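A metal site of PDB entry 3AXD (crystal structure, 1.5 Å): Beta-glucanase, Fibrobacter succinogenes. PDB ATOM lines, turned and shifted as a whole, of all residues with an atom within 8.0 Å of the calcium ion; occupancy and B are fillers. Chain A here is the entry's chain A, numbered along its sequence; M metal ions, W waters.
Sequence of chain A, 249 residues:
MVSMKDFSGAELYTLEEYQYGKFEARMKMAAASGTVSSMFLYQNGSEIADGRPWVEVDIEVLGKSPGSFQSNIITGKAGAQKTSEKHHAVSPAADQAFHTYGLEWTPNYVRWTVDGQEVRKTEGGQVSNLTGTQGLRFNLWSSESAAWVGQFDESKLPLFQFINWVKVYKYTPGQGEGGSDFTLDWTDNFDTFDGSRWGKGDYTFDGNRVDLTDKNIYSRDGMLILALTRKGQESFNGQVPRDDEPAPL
OD2 of Asp 191 sits at hydrogen-bond distance from ND2 of Asn 189 (2.9 Å). OD2 of Asp 243 is in hydrogen-bond range of ND2 of Asn 164 (2.9 Å). The backbone carbonyl oxygen (O) of Arg 26 lies within hydrogen-bond range of the backbone NH (N) of Asn 164.
Of the 17 residues printed, 3 come within 4 Å of the calcium ion.
The calcium ion is bound by water W2 (2.3 Å), the backbone carbonyl oxygen of Gly 222 (2.3 Å), the backbone carbonyl oxygen of Asn 189 (2.4 Å), water W3 (2.4 Å), the backbone carbonyl oxygen of Asn 164 (2.4 Å), the side-chain amide oxygen of Asn 164 (2.4 Å) and water W1 (2.6 Å).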
ATOM      1  N   ARG A  26      -8.584   3.618  -2.308  1.00  0.00           N
ATOM      2  CA  ARG A  26      -7.851   4.178  -1.169  1.00  0.00           C
ATOM      3  C   ARG A  26      -8.897   4.410  -0.096  1.00  0.00           C
ATOM      4  O   ARG A  26      -9.757   5.282  -0.230  1.00  0.00           O
ATOM      5  CB  ARG A  26      -7.240   5.515  -1.609  1.00  0.00           C
ATOM      6  CG  ARG A  26      -6.386   6.191  -0.574  1.00  0.00           C
ATOM      7  CD  ARG A  26      -5.168   5.365  -0.255  1.00  0.00           C
ATOM      8  NE  ARG A  26      -4.284   6.051   0.690  1.00  0.00           N
ATOM      9  CZ  ARG A  26      -3.156   5.543   1.163  1.00  0.00           C
ATOM     10  NH1 ARG A  26      -2.751   4.332   0.774  1.00  0.00           N
ATOM     11  NH2 ARG A  26      -2.441   6.225   2.045  1.00  0.00           N
ATOM     12  N   PHE A  98      -5.450   4.913   6.238  1.00  0.00           N
ATOM     13  CA  PHE A  98      -5.835   4.664   4.861  1.00  0.00           C
ATOM     14  C   PHE A  98      -4.890   3.618   4.283  1.00  0.00           C
ATOM     15  O   PHE A  98      -3.693   3.599   4.605  1.00  0.00           O
ATOM     16  CB  PHE A  98      -5.725   5.935   4.004  1.00  0.00           C
ATOM     17  CG  PHE A  98      -6.902   6.845   4.123  1.00  0.00           C
ATOM     18  CD1 PHE A  98      -6.948   7.803   5.131  1.00  0.00           C
ATOM     19  CD2 PHE A  98      -7.968   6.734   3.249  1.00  0.00           C
ATOM     20  CE1 PHE A  98      -8.060   8.636   5.264  1.00  0.00           C
ATOM     21  CE2 PHE A  98      -9.087   7.559   3.373  1.00  0.00           C
ATOM     22  CZ  PHE A  98      -9.133   8.517   4.370  1.00  0.00           C
ATOM     23  N   ILE A 163     -13.709   6.710   1.489  1.00  0.00           N
ATOM     24  CA  ILE A 163     -13.063   6.347   0.235  1.00  0.00           C
ATOM     25  C   ILE A 163     -12.490   7.633  -0.373  1.00  0.00           C
ATOM     26  O   ILE A 163     -13.242   8.561  -0.708  1.00  0.00           O
ATOM     27  CB  ILE A 163     -14.052   5.692  -0.773  1.00  0.00           C
ATOM     28  CG1 ILE A 163     -14.875   4.614  -0.068  1.00  0.00           C
ATOM     29  CG2 ILE A 163     -13.263   5.107  -1.945  1.00  0.00           C
ATOM     30  CD1 ILE A 163     -15.880   3.922  -0.965  1.00  0.00           C
ATOM     31  N   ASN A 164     -11.173   7.680  -0.503  1.00  0.00           N
ATOM     32  CA  ASN A 164     -10.488   8.872  -1.025  1.00  0.00           C
ATOM     33  C   ASN A 164     -10.406   8.931  -2.539  1.00  0.00           C
ATOM     34  O   ASN A 164     -10.497  10.015  -3.140  1.00  0.00           O
ATOM     35  CB  ASN A 164      -9.085   8.953  -0.404  1.00  0.00           C
ATOM     36  CG  ASN A 164      -8.464  10.318  -0.535  1.00  0.00           C
ATOM     37  OD1 ASN A 164      -9.123  11.278  -0.950  1.00  0.00           O
ATOM     38  ND2 ASN A 164      -7.206  10.437  -0.148  1.00  0.00           N
ATOM     39  N   TRP A 165     -10.210   7.780  -3.154  1.00  0.00           N
ATOM     40  CA  TRP A 165     -10.135   7.708  -4.601  1.00  0.00           C
ATOM     41  C   TRP A 165     -10.222   6.264  -5.038  1.00  0.00           C
ATOM     42  O   TRP A 165     -10.037   5.347  -4.233  1.00  0.00           O
ATOM     43  CB  TRP A 165      -8.858   8.371  -5.170  1.00  0.00           C
ATOM     44  CG  TRP A 165      -7.536   7.984  -4.559  1.00  0.00           C
ATOM     45  CD1 TRP A 165      -6.779   8.723  -3.678  1.00  0.00           C
ATOM     46  CD2 TRP A 165      -6.771   6.802  -4.843  1.00  0.00           C
ATOM     47  NE1 TRP A 165      -5.583   8.072  -3.408  1.00  0.00           N
ATOM     48  CE2 TRP A 165      -5.554   6.900  -4.116  1.00  0.00           C
ATOM     49  CE3 TRP A 165      -6.989   5.674  -5.647  1.00  0.00           C
ATOM     50  CZ2 TRP A 165      -4.562   5.908  -4.164  1.00  0.00           C
ATOM     51  CZ3 TRP A 165      -5.997   4.681  -5.695  1.00  0.00           C
ATOM     52  CH2 TRP A 165      -4.794   4.809  -4.949  1.00  0.00           C
ATOM     53  N   VAL A 166     -10.524   6.091  -6.317  1.00  0.00           N
ATOM     54  CA  VAL A 166     -10.652   4.781  -6.931  1.00  0.00           C
ATOM     55  C   VAL A 166      -9.999   4.802  -8.312  1.00  0.00           C
ATOM     56  O   VAL A 166     -10.017   5.825  -9.000  1.00  0.00           O
ATOM     57  CB  VAL A 166     -12.138   4.388  -7.079  1.00  0.00           C
ATOM     58  CG1 VAL A 166     -12.295   3.291  -8.144  1.00  0.00           C
ATOM     59  CG2 VAL A 166     -12.695   3.921  -5.736  1.00  0.00           C
ATOM     60  N   ASP A 188     -11.541   8.224 -10.005  1.00  0.00           N
ATOM     61  CA  ASP A 188     -12.486   9.131  -9.371  1.00  0.00           C
ATOM     62  C   ASP A 188     -11.839   9.598  -8.080  1.00  0.00           C
ATOM     63  O   ASP A 188     -11.464   8.760  -7.244  1.00  0.00           O
ATOM     64  CB  ASP A 188     -13.815   8.441  -9.063  1.00  0.00           C
ATOM     65  CG  ASP A 188     -14.938   9.429  -8.786  1.00  0.00           C
ATOM     66  OD1 ASP A 188     -14.652  10.538  -8.260  1.00  0.00           O
ATOM     67  OD2 ASP A 188     -16.097   9.102  -9.092  1.00  0.00           O
ATOM     68  N   ASN A 189     -11.697  10.908  -7.916  1.00  0.00           N
ATOM     69  CA  ASN A 189     -11.100  11.463  -6.699  1.00  0.00           C
ATOM     70  C   ASN A 189     -12.146  11.808  -5.641  1.00  0.00           C
ATOM     71  O   ASN A 189     -11.815  12.270  -4.555  1.00  0.00           O
ATOM     72  CB  ASN A 189     -10.242  12.702  -7.001  1.00  0.00           C
ATOM     73  CG  ASN A 189     -11.056  13.882  -7.548  1.00  0.00           C
ATOM     74  OD1 ASN A 189     -12.281  13.910  -7.491  1.00  0.00           O
ATOM     75  ND2 ASN A 189     -10.348  14.868  -8.091  1.00  0.00           N
ATOM     76  N   PHE A 190     -13.412  11.571  -5.973  1.00  0.00           N
ATOM     77  CA  PHE A 190     -14.525  11.822  -5.082  1.00  0.00           C
ATOM     78  C   PHE A 190     -14.708  13.238  -4.589  1.00  0.00           C
ATOM     79  O   PHE A 190     -15.153  13.470  -3.445  1.00  0.00           O
ATOM     80  CB  PHE A 190     -14.501  10.820  -3.915  1.00  0.00           C
ATOM     81  CG  PHE A 190     -14.750   9.411  -4.367  1.00  0.00           C
ATOM     82  CD1 PHE A 190     -15.939   9.075  -5.013  1.00  0.00           C
ATOM     83  CD2 PHE A 190     -13.769   8.434  -4.226  1.00  0.00           C
ATOM     84  CE1 PHE A 190     -16.139   7.799  -5.509  1.00  0.00           C
ATOM     85  CE2 PHE A 190     -13.962   7.150  -4.722  1.00  0.00           C
ATOM     86  CZ  PHE A 190     -15.151   6.828  -5.369  1.00  0.00           C
ATOM     87  N   ASP A 191     -14.362  14.193  -5.427  1.00  0.00           N
ATOM     88  CA  ASP A 191     -14.585  15.588  -5.063  1.00  0.00           C
ATOM     89  C   ASP A 191     -16.085  15.801  -5.128  1.00  0.00           C
ATOM     90  O   ASP A 191     -16.626  16.716  -4.518  1.00  0.00           O
ATOM     91  CB  ASP A 191     -13.890  16.533  -6.045  1.00  0.00           C
ATOM     92  CG  ASP A 191     -12.418  16.692  -5.756  1.00  0.00           C
ATOM     93  OD1 ASP A 191     -12.040  16.522  -4.571  1.00  0.00           O
ATOM     94  OD2 ASP A 191     -11.669  17.009  -6.689  1.00  0.00           O
ATOM     95  N   THR A 192     -16.765  14.934  -5.872  1.00  0.00           N
ATOM     96  CA  THR A 192     -18.206  15.001  -6.020  1.00  0.00           C
ATOM     97  C   THR A 192     -18.743  13.589  -6.166  1.00  0.00           C
ATOM     98  O   THR A 192     -17.970  12.641  -6.290  1.00  0.00           O
ATOM     99  CB  THR A 192     -18.615  15.776  -7.293  1.00  0.00           C
ATOM    100  OG1 THR A 192     -18.285  14.997  -8.454  1.00  0.00           O
ATOM    101  CG2 THR A 192     -17.889  17.123  -7.371  1.00  0.00           C
ATOM    102  N   ARG A 220     -17.963  14.656   1.178  1.00  0.00           N
ATOM    103  CA  ARG A 220     -17.398  15.777   1.918  1.00  0.00           C
ATOM    104  C   ARG A 220     -15.890  15.845   1.781  1.00  0.00           C
ATOM    105  O   ARG A 220     -15.197  14.828   1.869  1.00  0.00           O
ATOM    106  CB  ARG A 220     -17.734  15.672   3.409  1.00  0.00           C
ATOM    107  CG  ARG A 220     -19.201  15.414   3.756  1.00  0.00           C
ATOM    108  CD  ARG A 220     -20.104  16.604   3.456  1.00  0.00           C
ATOM    109  NE  ARG A 220     -21.514  16.303   3.746  1.00  0.00           N
ATOM    110  CZ  ARG A 220     -22.022  16.248   4.971  1.00  0.00           C
ATOM    111  NH1 ARG A 220     -21.264  16.486   6.035  1.00  0.00           N
ATOM    112  NH2 ARG A 220     -23.310  15.949   5.143  1.00  0.00           N
ATOM    113  N   ASP A 221     -15.387  17.043   1.566  1.00  0.00           N
ATOM    114  CA  ASP A 221     -13.959  17.304   1.468  1.00  0.00           C
ATOM    115  C   ASP A 221     -13.090  16.286   0.738  1.00  0.00           C
ATOM    116  O   ASP A 221     -12.097  15.787   1.278  1.00  0.00           O
ATOM    117  CB  ASP A 221     -13.419  17.542   2.879  1.00  0.00           C
ATOM    118  CG  ASP A 221     -14.204  18.617   3.617  1.00  0.00           C
ATOM    119  OD1 ASP A 221     -14.192  19.771   3.165  1.00  0.00           O
ATOM    120  OD2 ASP A 221     -14.834  18.298   4.652  1.00  0.00           O
ATOM    121  N   GLY A 222     -13.477  15.959  -0.485  1.00  0.00           N
ATOM    122  CA  GLY A 222     -12.678  15.037  -1.281  1.00  0.00           C
ATOM    123  C   GLY A 222     -12.881  13.560  -1.048  1.00  0.00           C
ATOM    124  O   GLY A 222     -12.151  12.742  -1.579  1.00  0.00           O
ATOM    125  N   MET A 223     -13.882  13.205  -0.268  1.00  0.00           N
ATOM    126  CA  MET A 223     -14.136  11.806  -0.029  1.00  0.00           C
ATOM    127  C   MET A 223     -15.567  11.362  -0.064  1.00  0.00           C
ATOM    128  O   MET A 223     -16.475  12.150   0.135  1.00  0.00           O
ATOM    129  CB  MET A 223     -13.496  11.380   1.263  1.00  0.00           C
ATOM    130  CG  MET A 223     -12.047  11.125   1.019  1.00  0.00           C
ATOM    131  SD  MET A 223     -11.295  10.522   2.430  1.00  0.00           S
ATOM    132  CE  MET A 223      -9.863  11.571   2.518  1.00  0.00           C
ATOM    133  N   LEU A 224     -15.743  10.079  -0.369  1.00  0.00           N
ATOM    134  CA  LEU A 224     -17.060   9.481  -0.395  1.00  0.00           C
ATOM    135  C   LEU A 224     -17.148   8.777   0.967  1.00  0.00           C
ATOM    136  O   LEU A 224     -16.256   8.008   1.337  1.00  0.00           O
ATOM    137  CB  LEU A 224     -17.145   8.479  -1.553  1.00  0.00           C
ATOM    138  CG  LEU A 224     -18.490   7.924  -2.022  1.00  0.00           C
ATOM    139  CD1 LEU A 224     -19.044   6.955  -0.986  1.00  0.00           C
ATOM    140  CD2 LEU A 224     -19.472   9.066  -2.280  1.00  0.00           C
ATOM    141  N   ASP A 243      -5.400  11.971   4.839  1.00  0.00           N
ATOM    142  CA  ASP A 243      -4.694  10.865   4.210  1.00  0.00           C
ATOM    143  C   ASP A 243      -3.301  11.436   3.938  1.00  0.00           C
ATOM    144  O   ASP A 243      -3.018  11.927   2.840  1.00  0.00           O
ATOM    145  CB  ASP A 243      -5.390  10.446   2.896  1.00  0.00           C
ATOM    146  CG  ASP A 243      -4.747   9.219   2.251  1.00  0.00           C
ATOM    147  OD1 ASP A 243      -3.755   8.721   2.821  1.00  0.00           O
ATOM    148  OD2 ASP A 243      -5.220   8.756   1.183  1.00  0.00           O
HETATM  149 CA    CA M   1     -10.211  12.396  -2.811  1.00  0.00          CA
HETATM  150  O   HOH W   1      -7.968  11.993  -3.956  1.00  0.00           O
HETATM  151  O   HOH W   2     -10.219  14.482  -3.797  1.00  0.00           O
HETATM  152  O   HOH W   3      -9.166  14.032  -1.405  1.00  0.00           O
